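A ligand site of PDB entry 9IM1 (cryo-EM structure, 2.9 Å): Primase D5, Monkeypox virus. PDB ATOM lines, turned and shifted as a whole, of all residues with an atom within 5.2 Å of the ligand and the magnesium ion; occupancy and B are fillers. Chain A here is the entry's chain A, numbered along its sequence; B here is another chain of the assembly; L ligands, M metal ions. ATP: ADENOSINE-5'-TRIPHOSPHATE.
The backbone NH (N) of Thr 507 is in hydrogen-bond range of an oxygen (O1B) of the ligand (2.9 Å).
The backbone NH (N) of Asp 652 lies within hydrogen-bond range of a nitrogen (N3) of the ligand (3.3 Å).
OG1 of Thr 505 is in hydrogen-bond range of O1G of the ligand (2.5 Å).
The side-chain amino group of Lys 509 lies within salt-bridge range of an oxygen (O1B) of the ligand, 3.0 Å away.
NH1 of Arg 619 of chain B is in salt-bridge range of O1G of the ligand (3.0 Å).
An oxygen (O1B) of the ligand is in hydrogen-bond range of the backbone NH (N) of Gly 508 (2.9 Å).
O2A of the ligand sits at hydrogen-bond distance from OG1 of Thr 511, at 3.0 Å.
N of Ser 510 lies within hydrogen-bond range of O2B of the ligand (3.0 Å).
An oxygen (O2A) of the ligand lies within hydrogen-bond range of the backbone NH of Thr 511, 3.5 Å away.
NH1 of Arg 620 of chain B lies within salt-bridge range of O1G of the ligand (3.7 Å).
N of Ala 506 sits at hydrogen-bond distance from O3B of the ligand.
N of Lys 509 lies within hydrogen-bond range of O1B of the ligand, 3.4 Å away.
OD1 of Asp 656 sits at hydrogen-bond distance from O2' of the ligand (3.0 Å).
The backbone carbonyl oxygen (O) of Ala 506 is in hydrogen-bond range of the backbone NH (N) of Phe 630 (3.3 Å).
The backbone carbonyl oxygen (O) of Thr 505 is in hydrogen-bond range of the side-chain hydroxyl (OG1) of Thr 507 (3.3 Å).
The side-chain hydroxyl (OG1) of Thr 507 is in hydrogen-bond range of the backbone carbonyl oxygen (O) of Glu 504.
The guanidinium group of Arg 620 of chain B sits at hydrogen-bond distance from the backbone carbonyl oxygen of Ala 616 of chain B (3.0 Å).
The side-chain amino group (NZ) of Lys 509 lies within hydrogen-bond range of the backbone carbonyl oxygen (O) of Glu 504, 3.1 Å away.
The side-chain hydroxyl (OG1) of Thr 505 lies within hydrogen-bond range of the guanidinium group (NH1) of Arg 619 of chain B (3.0 Å).
The side-chain amino group of Lys 649 lies within salt-bridge range of the side-chain carboxylate of Asp 467 (3.7 Å).
CA of Ile 464 touches N6 of the ligand, 3.8 Å away.
Asp 467 touches the ligand (CB to N6, 3.5 Å).
Glu 504 touches the ligand.
Asn 605 touches the ligand (ND2 to O2G, 3.7 Å).
CE1 of Phe 630 touches C6 of the ligand, 3.5 Å away.
Leu 650 touches the ligand (O to C2, 3.7 Å).
Leu 651 touches the ligand.
CB of Leu 655 touches O2' of the ligand, 3.8 Å away.
Hydrophobic or aromatic side chains within 4 Å of the ligand: Ile 464, Phe 630, Leu 651 and Leu 655.
19 residues have an atom within 4 Å of the ligand: Ile 464, Asp 467, Glu 504, Thr 505, Ala 506, Thr 507, Gly 508, Lys 509, Ser 510, Thr 511, Asn 605, Phe 630, Leu 650, Leu 651, Asp 652, Leu 655, Asp 656, Arg 619 of chain B and Arg 620 of chain B.
The nearest printed residue that does not touch the ligand is Lys 649 (4.1 Å).
The nearest printed residue that does not touch the magnesium ion is Glu 579 of chain B (4.04 Å).
The magnesium ion is bound by O3G of the ligand (2.1 Å) and OG of Ser 510 (2.3 Å).
Slightly farther from the magnesium ion lies an oxygen (O2B) of the ligand (2.7 Å).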
ATOM      1  N   ASN A 463     -25.597  -4.422  -6.428  1.00  0.00           N
ATOM      2  CA  ASN A 463     -26.329  -3.573  -7.365  1.00  0.00           C
ATOM      3  C   ASN A 463     -25.740  -3.660  -8.770  1.00  0.00           C
ATOM      4  O   ASN A 463     -26.484  -3.758  -9.758  1.00  0.00           O
ATOM      5  CB  ASN A 463     -26.321  -2.118  -6.875  1.00  0.00           C
ATOM      6  CG  ASN A 463     -26.894  -1.980  -5.480  1.00  0.00           C
ATOM      7  OD1 ASN A 463     -27.474  -2.916  -4.941  1.00  0.00           O
ATOM      8  ND2 ASN A 463     -26.745  -0.797  -4.899  1.00  0.00           N
ATOM      9  N   ILE A 464     -24.417  -3.663  -8.880  1.00  0.00           N
ATOM     10  CA  ILE A 464     -23.769  -3.739 -10.184  1.00  0.00           C
ATOM     11  C   ILE A 464     -24.088  -5.074 -10.853  1.00  0.00           C
ATOM     12  O   ILE A 464     -24.408  -5.126 -12.050  1.00  0.00           O
ATOM     13  CB  ILE A 464     -22.250  -3.534 -10.038  1.00  0.00           C
ATOM     14  CG1 ILE A 464     -21.949  -2.099  -9.601  1.00  0.00           C
ATOM     15  CG2 ILE A 464     -21.537  -3.853 -11.343  1.00  0.00           C
ATOM     16  CD1 ILE A 464     -20.481  -1.835  -9.381  1.00  0.00           C
ATOM     17  N   ASP A 467     -27.519  -5.166 -12.076  1.00  0.00           N
ATOM     18  CA  ASP A 467     -27.643  -4.313 -13.247  1.00  0.00           C
ATOM     19  C   ASP A 467     -27.157  -5.019 -14.505  1.00  0.00           C
ATOM     20  O   ASP A 467     -27.801  -4.929 -15.553  1.00  0.00           O
ATOM     21  CB  ASP A 467     -26.867  -3.017 -13.032  1.00  0.00           C
ATOM     22  CG  ASP A 467     -27.684  -1.955 -12.325  1.00  0.00           C
ATOM     23  OD1 ASP A 467     -28.871  -2.226 -12.024  1.00  0.00           O
ATOM     24  OD2 ASP A 467     -27.137  -0.867 -12.062  1.00  0.00           O
ATOM     25  N   ILE A 468     -26.032  -5.718 -14.416  1.00  0.00           N
ATOM     26  CA  ILE A 468     -25.486  -6.390 -15.601  1.00  0.00           C
ATOM     27  C   ILE A 468     -26.363  -7.571 -15.991  1.00  0.00           C
ATOM     28  O   ILE A 468     -26.661  -7.766 -17.181  1.00  0.00           O
ATOM     29  CB  ILE A 468     -24.037  -6.830 -15.348  1.00  0.00           C
ATOM     30  CG1 ILE A 468     -23.155  -5.605 -15.061  1.00  0.00           C
ATOM     31  CG2 ILE A 468     -23.503  -7.593 -16.537  1.00  0.00           C
ATOM     32  CD1 ILE A 468     -21.694  -5.945 -14.882  1.00  0.00           C
ATOM     33  N   GLU A 504     -23.425  -6.695 -27.551  1.00  0.00           N
ATOM     34  CA  GLU A 504     -23.121  -5.508 -28.327  1.00  0.00           C
ATOM     35  C   GLU A 504     -22.209  -4.604 -27.491  1.00  0.00           C
ATOM     36  O   GLU A 504     -21.763  -4.966 -26.404  1.00  0.00           O
ATOM     37  CB  GLU A 504     -24.417  -4.818 -28.752  1.00  0.00           C
ATOM     38  CG  GLU A 504     -24.284  -3.923 -29.981  1.00  0.00           C
ATOM     39  CD  GLU A 504     -24.119  -4.709 -31.268  1.00  0.00           C
ATOM     40  OE1 GLU A 504     -24.852  -5.702 -31.443  1.00  0.00           O
ATOM     41  OE2 GLU A 504     -23.258  -4.333 -32.095  1.00  0.00           O
ATOM     42  N   THR A 505     -21.913  -3.406 -28.004  1.00  0.00           N
ATOM     43  CA  THR A 505     -20.980  -2.521 -27.320  1.00  0.00           C
ATOM     44  C   THR A 505     -21.590  -1.937 -26.057  1.00  0.00           C
ATOM     45  O   THR A 505     -22.819  -1.818 -25.919  1.00  0.00           O
ATOM     46  CB  THR A 505     -20.526  -1.399 -28.263  1.00  0.00           C
ATOM     47  OG1 THR A 505     -19.261  -0.899 -27.829  1.00  0.00           O
ATOM     48  CG2 THR A 505     -21.541  -0.255 -28.277  1.00  0.00           C
ATOM     49  N   ALA A 506     -20.722  -1.587 -25.107  1.00  0.00           N
ATOM     50  CA  ALA A 506     -21.097  -0.946 -23.847  1.00  0.00           C
ATOM     51  C   ALA A 506     -22.155  -1.769 -23.102  1.00  0.00           C
ATOM     52  O   ALA A 506     -23.275  -1.327 -22.849  1.00  0.00           O
ATOM     53  CB  ALA A 506     -21.591   0.489 -24.091  1.00  0.00           C
ATOM     54  N   THR A 507     -21.765  -2.994 -22.762  1.00  0.00           N
ATOM     55  CA  THR A 507     -22.677  -3.928 -22.111  1.00  0.00           C
ATOM     56  C   THR A 507     -22.192  -4.425 -20.759  1.00  0.00           C
ATOM     57  O   THR A 507     -23.022  -4.772 -19.910  1.00  0.00           O
ATOM     58  CB  THR A 507     -22.938  -5.135 -23.024  1.00  0.00           C
ATOM     59  OG1 THR A 507     -23.072  -4.675 -24.372  1.00  0.00           O
ATOM     60  CG2 THR A 507     -24.211  -5.829 -22.623  1.00  0.00           C
ATOM     61  N   GLY A 508     -20.878  -4.459 -20.520  1.00  0.00           N
ATOM     62  CA  GLY A 508     -20.376  -4.817 -19.208  1.00  0.00           C
ATOM     63  C   GLY A 508     -19.537  -6.080 -19.161  1.00  0.00           C
ATOM     64  O   GLY A 508     -19.334  -6.646 -18.085  1.00  0.00           O
ATOM     65  N   LYS A 509     -19.061  -6.544 -20.320  1.00  0.00           N
ATOM     66  CA  LYS A 509     -18.215  -7.733 -20.332  1.00  0.00           C
ATOM     67  C   LYS A 509     -16.834  -7.433 -19.773  1.00  0.00           C
ATOM     68  O   LYS A 509     -16.301  -8.224 -18.971  1.00  0.00           O
ATOM     69  CB  LYS A 509     -18.117  -8.266 -21.762  1.00  0.00           C
ATOM     70  CG  LYS A 509     -19.452  -8.626 -22.379  1.00  0.00           C
ATOM     71  CD  LYS A 509     -19.291  -9.137 -23.802  1.00  0.00           C
ATOM     72  CE  LYS A 509     -18.921  -8.026 -24.758  1.00  0.00           C
ATOM     73  NZ  LYS A 509     -20.040  -7.059 -24.940  1.00  0.00           N
ATOM     74  N   SER A 510     -16.239  -6.309 -20.166  1.00  0.00           N
ATOM     75  CA  SER A 510     -14.928  -5.940 -19.651  1.00  0.00           C
ATOM     76  C   SER A 510     -14.975  -5.700 -18.145  1.00  0.00           C
ATOM     77  O   SER A 510     -14.005  -6.014 -17.439  1.00  0.00           O
ATOM     78  CB  SER A 510     -14.413  -4.695 -20.370  1.00  0.00           C
ATOM     79  OG  SER A 510     -14.122  -4.973 -21.722  1.00  0.00           O
ATOM     80  N   THR A 511     -16.072  -5.154 -17.638  1.00  0.00           N
ATOM     81  CA  THR A 511     -16.210  -4.975 -16.197  1.00  0.00           C
ATOM     82  C   THR A 511     -16.146  -6.310 -15.469  1.00  0.00           C
ATOM     83  O   THR A 511     -15.466  -6.438 -14.445  1.00  0.00           O
ATOM     84  CB  THR A 511     -17.513  -4.248 -15.884  1.00  0.00           C
ATOM     85  OG1 THR A 511     -17.521  -2.970 -16.522  1.00  0.00           O
ATOM     86  CG2 THR A 511     -17.661  -4.052 -14.384  1.00  0.00           C
ATOM     87  N   GLU A 557     -11.795  -9.719 -28.463  1.00  0.00           N
ATOM     88  CA  GLU A 557     -11.934  -9.058 -29.754  1.00  0.00           C
ATOM     89  C   GLU A 557     -11.740 -10.023 -30.920  1.00  0.00           C
ATOM     90  O   GLU A 557     -10.792  -9.922 -31.702  1.00  0.00           O
ATOM     91  CB  GLU A 557     -10.969  -7.867 -29.843  1.00  0.00           C
ATOM     92  CG  GLU A 557     -11.233  -6.713 -28.857  1.00  0.00           C
ATOM     93  CD  GLU A 557     -12.675  -6.550 -28.377  1.00  0.00           C
ATOM     94  OE1 GLU A 557     -13.635  -6.814 -29.136  1.00  0.00           O
ATOM     95  OE2 GLU A 557     -12.855  -6.163 -27.197  1.00  0.00           O
ATOM     96  N   ASP A 603     -14.508 -13.106 -25.154  1.00  0.00           N
ATOM     97  CA  ASP A 603     -15.559 -12.101 -25.266  1.00  0.00           C
ATOM     98  C   ASP A 603     -15.527 -11.461 -26.644  1.00  0.00           C
ATOM     99  O   ASP A 603     -14.469 -11.028 -27.125  1.00  0.00           O
ATOM    100  CB  ASP A 603     -15.471 -11.039 -24.171  1.00  0.00           C
ATOM    101  CG  ASP A 603     -14.136 -10.327 -24.134  1.00  0.00           C
ATOM    102  OD1 ASP A 603     -13.999  -9.401 -23.312  1.00  0.00           O
ATOM    103  OD2 ASP A 603     -13.207 -10.696 -24.866  1.00  0.00           O
ATOM    104  N   ASN A 605     -18.143  -9.646 -30.111  1.00  0.00           N
ATOM    105  CA  ASN A 605     -19.371  -9.047 -30.615  1.00  0.00           C
ATOM    106  C   ASN A 605     -19.948  -9.806 -31.798  1.00  0.00           C
ATOM    107  O   ASN A 605     -21.028  -9.440 -32.291  1.00  0.00           O
ATOM    108  CB  ASN A 605     -19.134  -7.593 -31.011  1.00  0.00           C
ATOM    109  CG  ASN A 605     -18.746  -6.726 -29.842  1.00  0.00           C
ATOM    110  OD1 ASN A 605     -17.638  -6.212 -29.768  1.00  0.00           O
ATOM    111  ND2 ASN A 605     -19.678  -6.546 -28.902  1.00  0.00           N
ATOM    112  N   PHE A 630     -25.340   0.553 -21.103  1.00  0.00           N
ATOM    113  CA  PHE A 630     -25.022   1.741 -20.314  1.00  0.00           C
ATOM    114  C   PHE A 630     -24.645   2.857 -21.273  1.00  0.00           C
ATOM    115  O   PHE A 630     -23.709   2.709 -22.071  1.00  0.00           O
ATOM    116  CB  PHE A 630     -23.895   1.455 -19.334  1.00  0.00           C
ATOM    117  CG  PHE A 630     -24.150   0.266 -18.443  1.00  0.00           C
ATOM    118  CD1 PHE A 630     -24.990   0.374 -17.351  1.00  0.00           C
ATOM    119  CD2 PHE A 630     -23.563  -0.952 -18.709  1.00  0.00           C
ATOM    120  CE1 PHE A 630     -25.239  -0.712 -16.541  1.00  0.00           C
ATOM    121  CE2 PHE A 630     -23.796  -2.045 -17.901  1.00  0.00           C
ATOM    122  CZ  PHE A 630     -24.635  -1.921 -16.814  1.00  0.00           C
ATOM    123  N   LYS A 649     -29.407   2.204 -18.846  1.00  0.00           N
ATOM    124  CA  LYS A 649     -29.139   2.876 -17.581  1.00  0.00           C
ATOM    125  C   LYS A 649     -27.951   3.811 -17.771  1.00  0.00           C
ATOM    126  O   LYS A 649     -27.102   3.588 -18.647  1.00  0.00           O
ATOM    127  CB  LYS A 649     -28.873   1.863 -16.461  1.00  0.00           C
ATOM    128  CG  LYS A 649     -28.671   2.472 -15.086  1.00  0.00           C
ATOM    129  CD  LYS A 649     -28.474   1.403 -14.031  1.00  0.00           C
ATOM    130  CE  LYS A 649     -28.363   2.033 -12.644  1.00  0.00           C
ATOM    131  NZ  LYS A 649     -27.129   2.837 -12.490  1.00  0.00           N
ATOM    132  N   LEU A 650     -27.888   4.849 -16.950  1.00  0.00           N
ATOM    133  CA  LEU A 650     -26.818   5.830 -17.037  1.00  0.00           C
ATOM    134  C   LEU A 650     -25.470   5.206 -16.694  1.00  0.00           C
ATOM    135  O   LEU A 650     -25.377   4.268 -15.886  1.00  0.00           O
ATOM    136  CB  LEU A 650     -27.081   7.005 -16.109  1.00  0.00           C
ATOM    137  CG  LEU A 650     -28.278   7.902 -16.455  1.00  0.00           C
ATOM    138  CD1 LEU A 650     -28.503   8.932 -15.365  1.00  0.00           C
ATOM    139  CD2 LEU A 650     -28.059   8.566 -17.792  1.00  0.00           C
ATOM    140  N   LEU A 651     -24.425   5.726 -17.322  1.00  0.00           N
ATOM    141  CA  LEU A 651     -23.072   5.250 -17.117  1.00  0.00           C
ATOM    142  C   LEU A 651     -22.430   5.940 -15.927  1.00  0.00           C
ATOM    143  O   LEU A 651     -22.700   7.111 -15.637  1.00  0.00           O
ATOM    144  CB  LEU A 651     -22.224   5.488 -18.366  1.00  0.00           C
ATOM    145  CG  LEU A 651     -20.823   4.881 -18.458  1.00  0.00           C
ATOM    146  CD1 LEU A 651     -20.549   4.398 -19.866  1.00  0.00           C
ATOM    147  CD2 LEU A 651     -19.771   5.890 -18.026  1.00  0.00           C
ATOM    148  N   ASP A 652     -21.582   5.199 -15.208  1.00  0.00           N
ATOM    149  CA  ASP A 652     -20.834   5.725 -14.074  1.00  0.00           C
ATOM    150  C   ASP A 652     -19.378   5.907 -14.494  1.00  0.00           C
ATOM    151  O   ASP A 652     -18.730   4.942 -14.916  1.00  0.00           O
ATOM    152  CB  ASP A 652     -20.945   4.791 -12.872  1.00  0.00           C
ATOM    153  CG  ASP A 652     -20.429   5.422 -11.595  1.00  0.00           C
ATOM    154  OD1 ASP A 652     -20.179   6.647 -11.596  1.00  0.00           O
ATOM    155  OD2 ASP A 652     -20.276   4.695 -10.593  1.00  0.00           O
ATOM    156  N   LEU A 655     -16.383   4.211 -11.952  1.00  0.00           N
ATOM    157  CA  LEU A 655     -16.391   2.799 -11.592  1.00  0.00           C
ATOM    158  C   LEU A 655     -15.076   2.125 -11.952  1.00  0.00           C
ATOM    159  O   LEU A 655     -14.579   1.275 -11.201  1.00  0.00           O
ATOM    160  CB  LEU A 655     -17.563   2.085 -12.269  1.00  0.00           C
ATOM    161  CG  LEU A 655     -17.780   0.637 -11.843  1.00  0.00           C
ATOM    162  CD1 LEU A 655     -17.927   0.561 -10.328  1.00  0.00           C
ATOM    163  CD2 LEU A 655     -18.997   0.061 -12.528  1.00  0.00           C
ATOM    164  N   ASP A 656     -14.499   2.483 -13.105  1.00  0.00           N
ATOM    165  CA  ASP A 656     -13.264   1.827 -13.547  1.00  0.00           C
ATOM    166  C   ASP A 656     -12.112   2.117 -12.583  1.00  0.00           C
ATOM    167  O   ASP A 656     -11.310   1.226 -12.297  1.00  0.00           O
ATOM    168  CB  ASP A 656     -12.910   2.284 -14.958  1.00  0.00           C
ATOM    169  CG  ASP A 656     -14.112   2.257 -15.892  1.00  0.00           C
ATOM    170  OD1 ASP A 656     -14.592   1.146 -16.204  1.00  0.00           O
ATOM    171  OD2 ASP A 656     -14.574   3.340 -16.304  1.00  0.00           O
ATOM    172  N   GLU B 579      -7.645  -1.494 -24.743  1.00  0.00           N
ATOM    173  CA  GLU B 579      -7.643  -2.258 -23.509  1.00  0.00           C
ATOM    174  C   GLU B 579      -6.396  -1.932 -22.678  1.00  0.00           C
ATOM    175  O   GLU B 579      -5.356  -1.581 -23.224  1.00  0.00           O
ATOM    176  CB  GLU B 579      -7.694  -3.755 -23.809  1.00  0.00           C
ATOM    177  CG  GLU B 579      -8.677  -4.153 -24.897  1.00  0.00           C
ATOM    178  CD  GLU B 579     -10.135  -4.103 -24.460  1.00  0.00           C
ATOM    179  OE1 GLU B 579     -10.530  -3.188 -23.702  1.00  0.00           O
ATOM    180  OE2 GLU B 579     -10.906  -4.992 -24.878  1.00  0.00           O
ATOM    181  N   ALA B 616     -19.282  -0.306 -31.843  1.00  0.00           N
ATOM    182  CA  ALA B 616     -18.077  -0.369 -31.023  1.00  0.00           C
ATOM    183  C   ALA B 616     -16.924   0.408 -31.632  1.00  0.00           C
ATOM    184  O   ALA B 616     -16.046   0.892 -30.915  1.00  0.00           O
ATOM    185  CB  ALA B 616     -17.678  -1.831 -30.807  1.00  0.00           C
ATOM    186  N   ARG B 619     -17.204   4.680 -31.190  1.00  0.00           N
ATOM    187  CA  ARG B 619     -16.970   5.300 -29.902  1.00  0.00           C
ATOM    188  C   ARG B 619     -15.498   5.307 -29.519  1.00  0.00           C
ATOM    189  O   ARG B 619     -15.170   5.388 -28.324  1.00  0.00           O
ATOM    190  CB  ARG B 619     -17.791   4.582 -28.825  1.00  0.00           C
ATOM    191  CG  ARG B 619     -17.617   3.076 -28.800  1.00  0.00           C
ATOM    192  CD  ARG B 619     -18.237   2.469 -27.557  1.00  0.00           C
ATOM    193  NE  ARG B 619     -17.308   2.449 -26.432  1.00  0.00           N
ATOM    194  CZ  ARG B 619     -17.317   1.530 -25.465  1.00  0.00           C
ATOM    195  NH1 ARG B 619     -18.187   0.537 -25.467  1.00  0.00           N
ATOM    196  NH2 ARG B 619     -16.421   1.610 -24.491  1.00  0.00           N
ATOM    197  N   ARG B 620     -14.595   5.240 -30.494  1.00  0.00           N
ATOM    198  CA  ARG B 620     -13.163   5.182 -30.206  1.00  0.00           C
ATOM    199  C   ARG B 620     -12.332   6.032 -31.168  1.00  0.00           C
ATOM    200  O   ARG B 620     -11.123   5.796 -31.278  1.00  0.00           O
ATOM    201  CB  ARG B 620     -12.663   3.741 -30.248  1.00  0.00           C
ATOM    202  CG  ARG B 620     -13.185   2.851 -29.126  1.00  0.00           C
ATOM    203  CD  ARG B 620     -12.872   1.402 -29.395  1.00  0.00           C
ATOM    204  NE  ARG B 620     -12.800   0.612 -28.174  1.00  0.00           N
ATOM    205  CZ  ARG B 620     -13.778  -0.156 -27.720  1.00  0.00           C
ATOM    206  NH1 ARG B 620     -14.918  -0.278 -28.368  1.00  0.00           N
ATOM    207  NH2 ARG B 620     -13.596  -0.838 -26.586  1.00  0.00           N
HETATM  208  PG  ATP L   1     -17.342  -3.368 -25.696  1.00  0.00           P
HETATM  209  O1G ATP L   1     -17.512  -2.148 -26.540  1.00  0.00           O
HETATM  210  O2G ATP L   1     -18.087  -4.591 -26.239  1.00  0.00           O
HETATM  211  O3G ATP L   1     -15.880  -3.742 -25.441  1.00  0.00           O
HETATM  212  PB  ATP L   1     -18.330  -3.960 -22.938  1.00  0.00           P
HETATM  213  O1B ATP L   1     -19.556  -4.761 -23.126  1.00  0.00           O
HETATM  214  O2B ATP L   1     -17.093  -4.736 -22.535  1.00  0.00           O
HETATM  215  O3B ATP L   1     -17.969  -3.133 -24.242  1.00  0.00           O
HETATM  216  PA  ATP L   1     -17.634  -2.044 -20.807  1.00  0.00           P
HETATM  217  O1A ATP L   1     -16.241  -1.905 -21.289  1.00  0.00           O
HETATM  218  O2A ATP L   1     -17.791  -2.779 -19.477  1.00  0.00           O
HETATM  219  O3A ATP L   1     -18.529  -2.800 -21.873  1.00  0.00           O
HETATM  220  O5' ATP L   1     -18.329  -0.639 -20.695  1.00  0.00           O
HETATM  221  C5' ATP L   1     -19.442  -0.423 -19.791  1.00  0.00           C
HETATM  222  C4' ATP L   1     -19.306   0.960 -19.205  1.00  0.00           C
HETATM  223  O4' ATP L   1     -20.360   1.175 -18.248  1.00  0.00           O
HETATM  224  C3' ATP L   1     -18.017   1.206 -18.441  1.00  0.00           C
HETATM  225  O3' ATP L   1     -17.654   2.586 -18.489  1.00  0.00           O
HETATM  226  C2' ATP L   1     -18.374   0.765 -17.017  1.00  0.00           C
HETATM  227  O2' ATP L   1     -17.598   1.442 -16.050  1.00  0.00           O
HETATM  228  C1' ATP L   1     -19.839   1.202 -16.926  1.00  0.00           C
HETATM  229  N9  ATP L   1     -20.662   0.328 -16.096  1.00  0.00           N
HETATM  230  C8  ATP L   1     -20.590  -1.034 -16.004  1.00  0.00           C
HETATM  231  N7  ATP L   1     -21.448  -1.566 -15.176  1.00  0.00           N
HETATM  232  C5  ATP L   1     -22.153  -0.472 -14.687  1.00  0.00           C
HETATM  233  C6  ATP L   1     -23.205  -0.349 -13.761  1.00  0.00           C
HETATM  234  N6  ATP L   1     -23.775  -1.397 -13.144  1.00  0.00           N
HETATM  235  N1  ATP L   1     -23.667   0.886 -13.496  1.00  0.00           N
HETATM  236  C2  ATP L   1     -23.110   1.933 -14.116  1.00  0.00           C
HETATM  237  N3  ATP L   1     -22.117   1.944 -15.000  1.00  0.00           N
HETATM  238  C4  ATP L   1     -21.676   0.699 -15.242  1.00  0.00           C
HETATM  239 MG    MG M   1     -14.772  -4.503 -23.829  1.00  0.00          MG
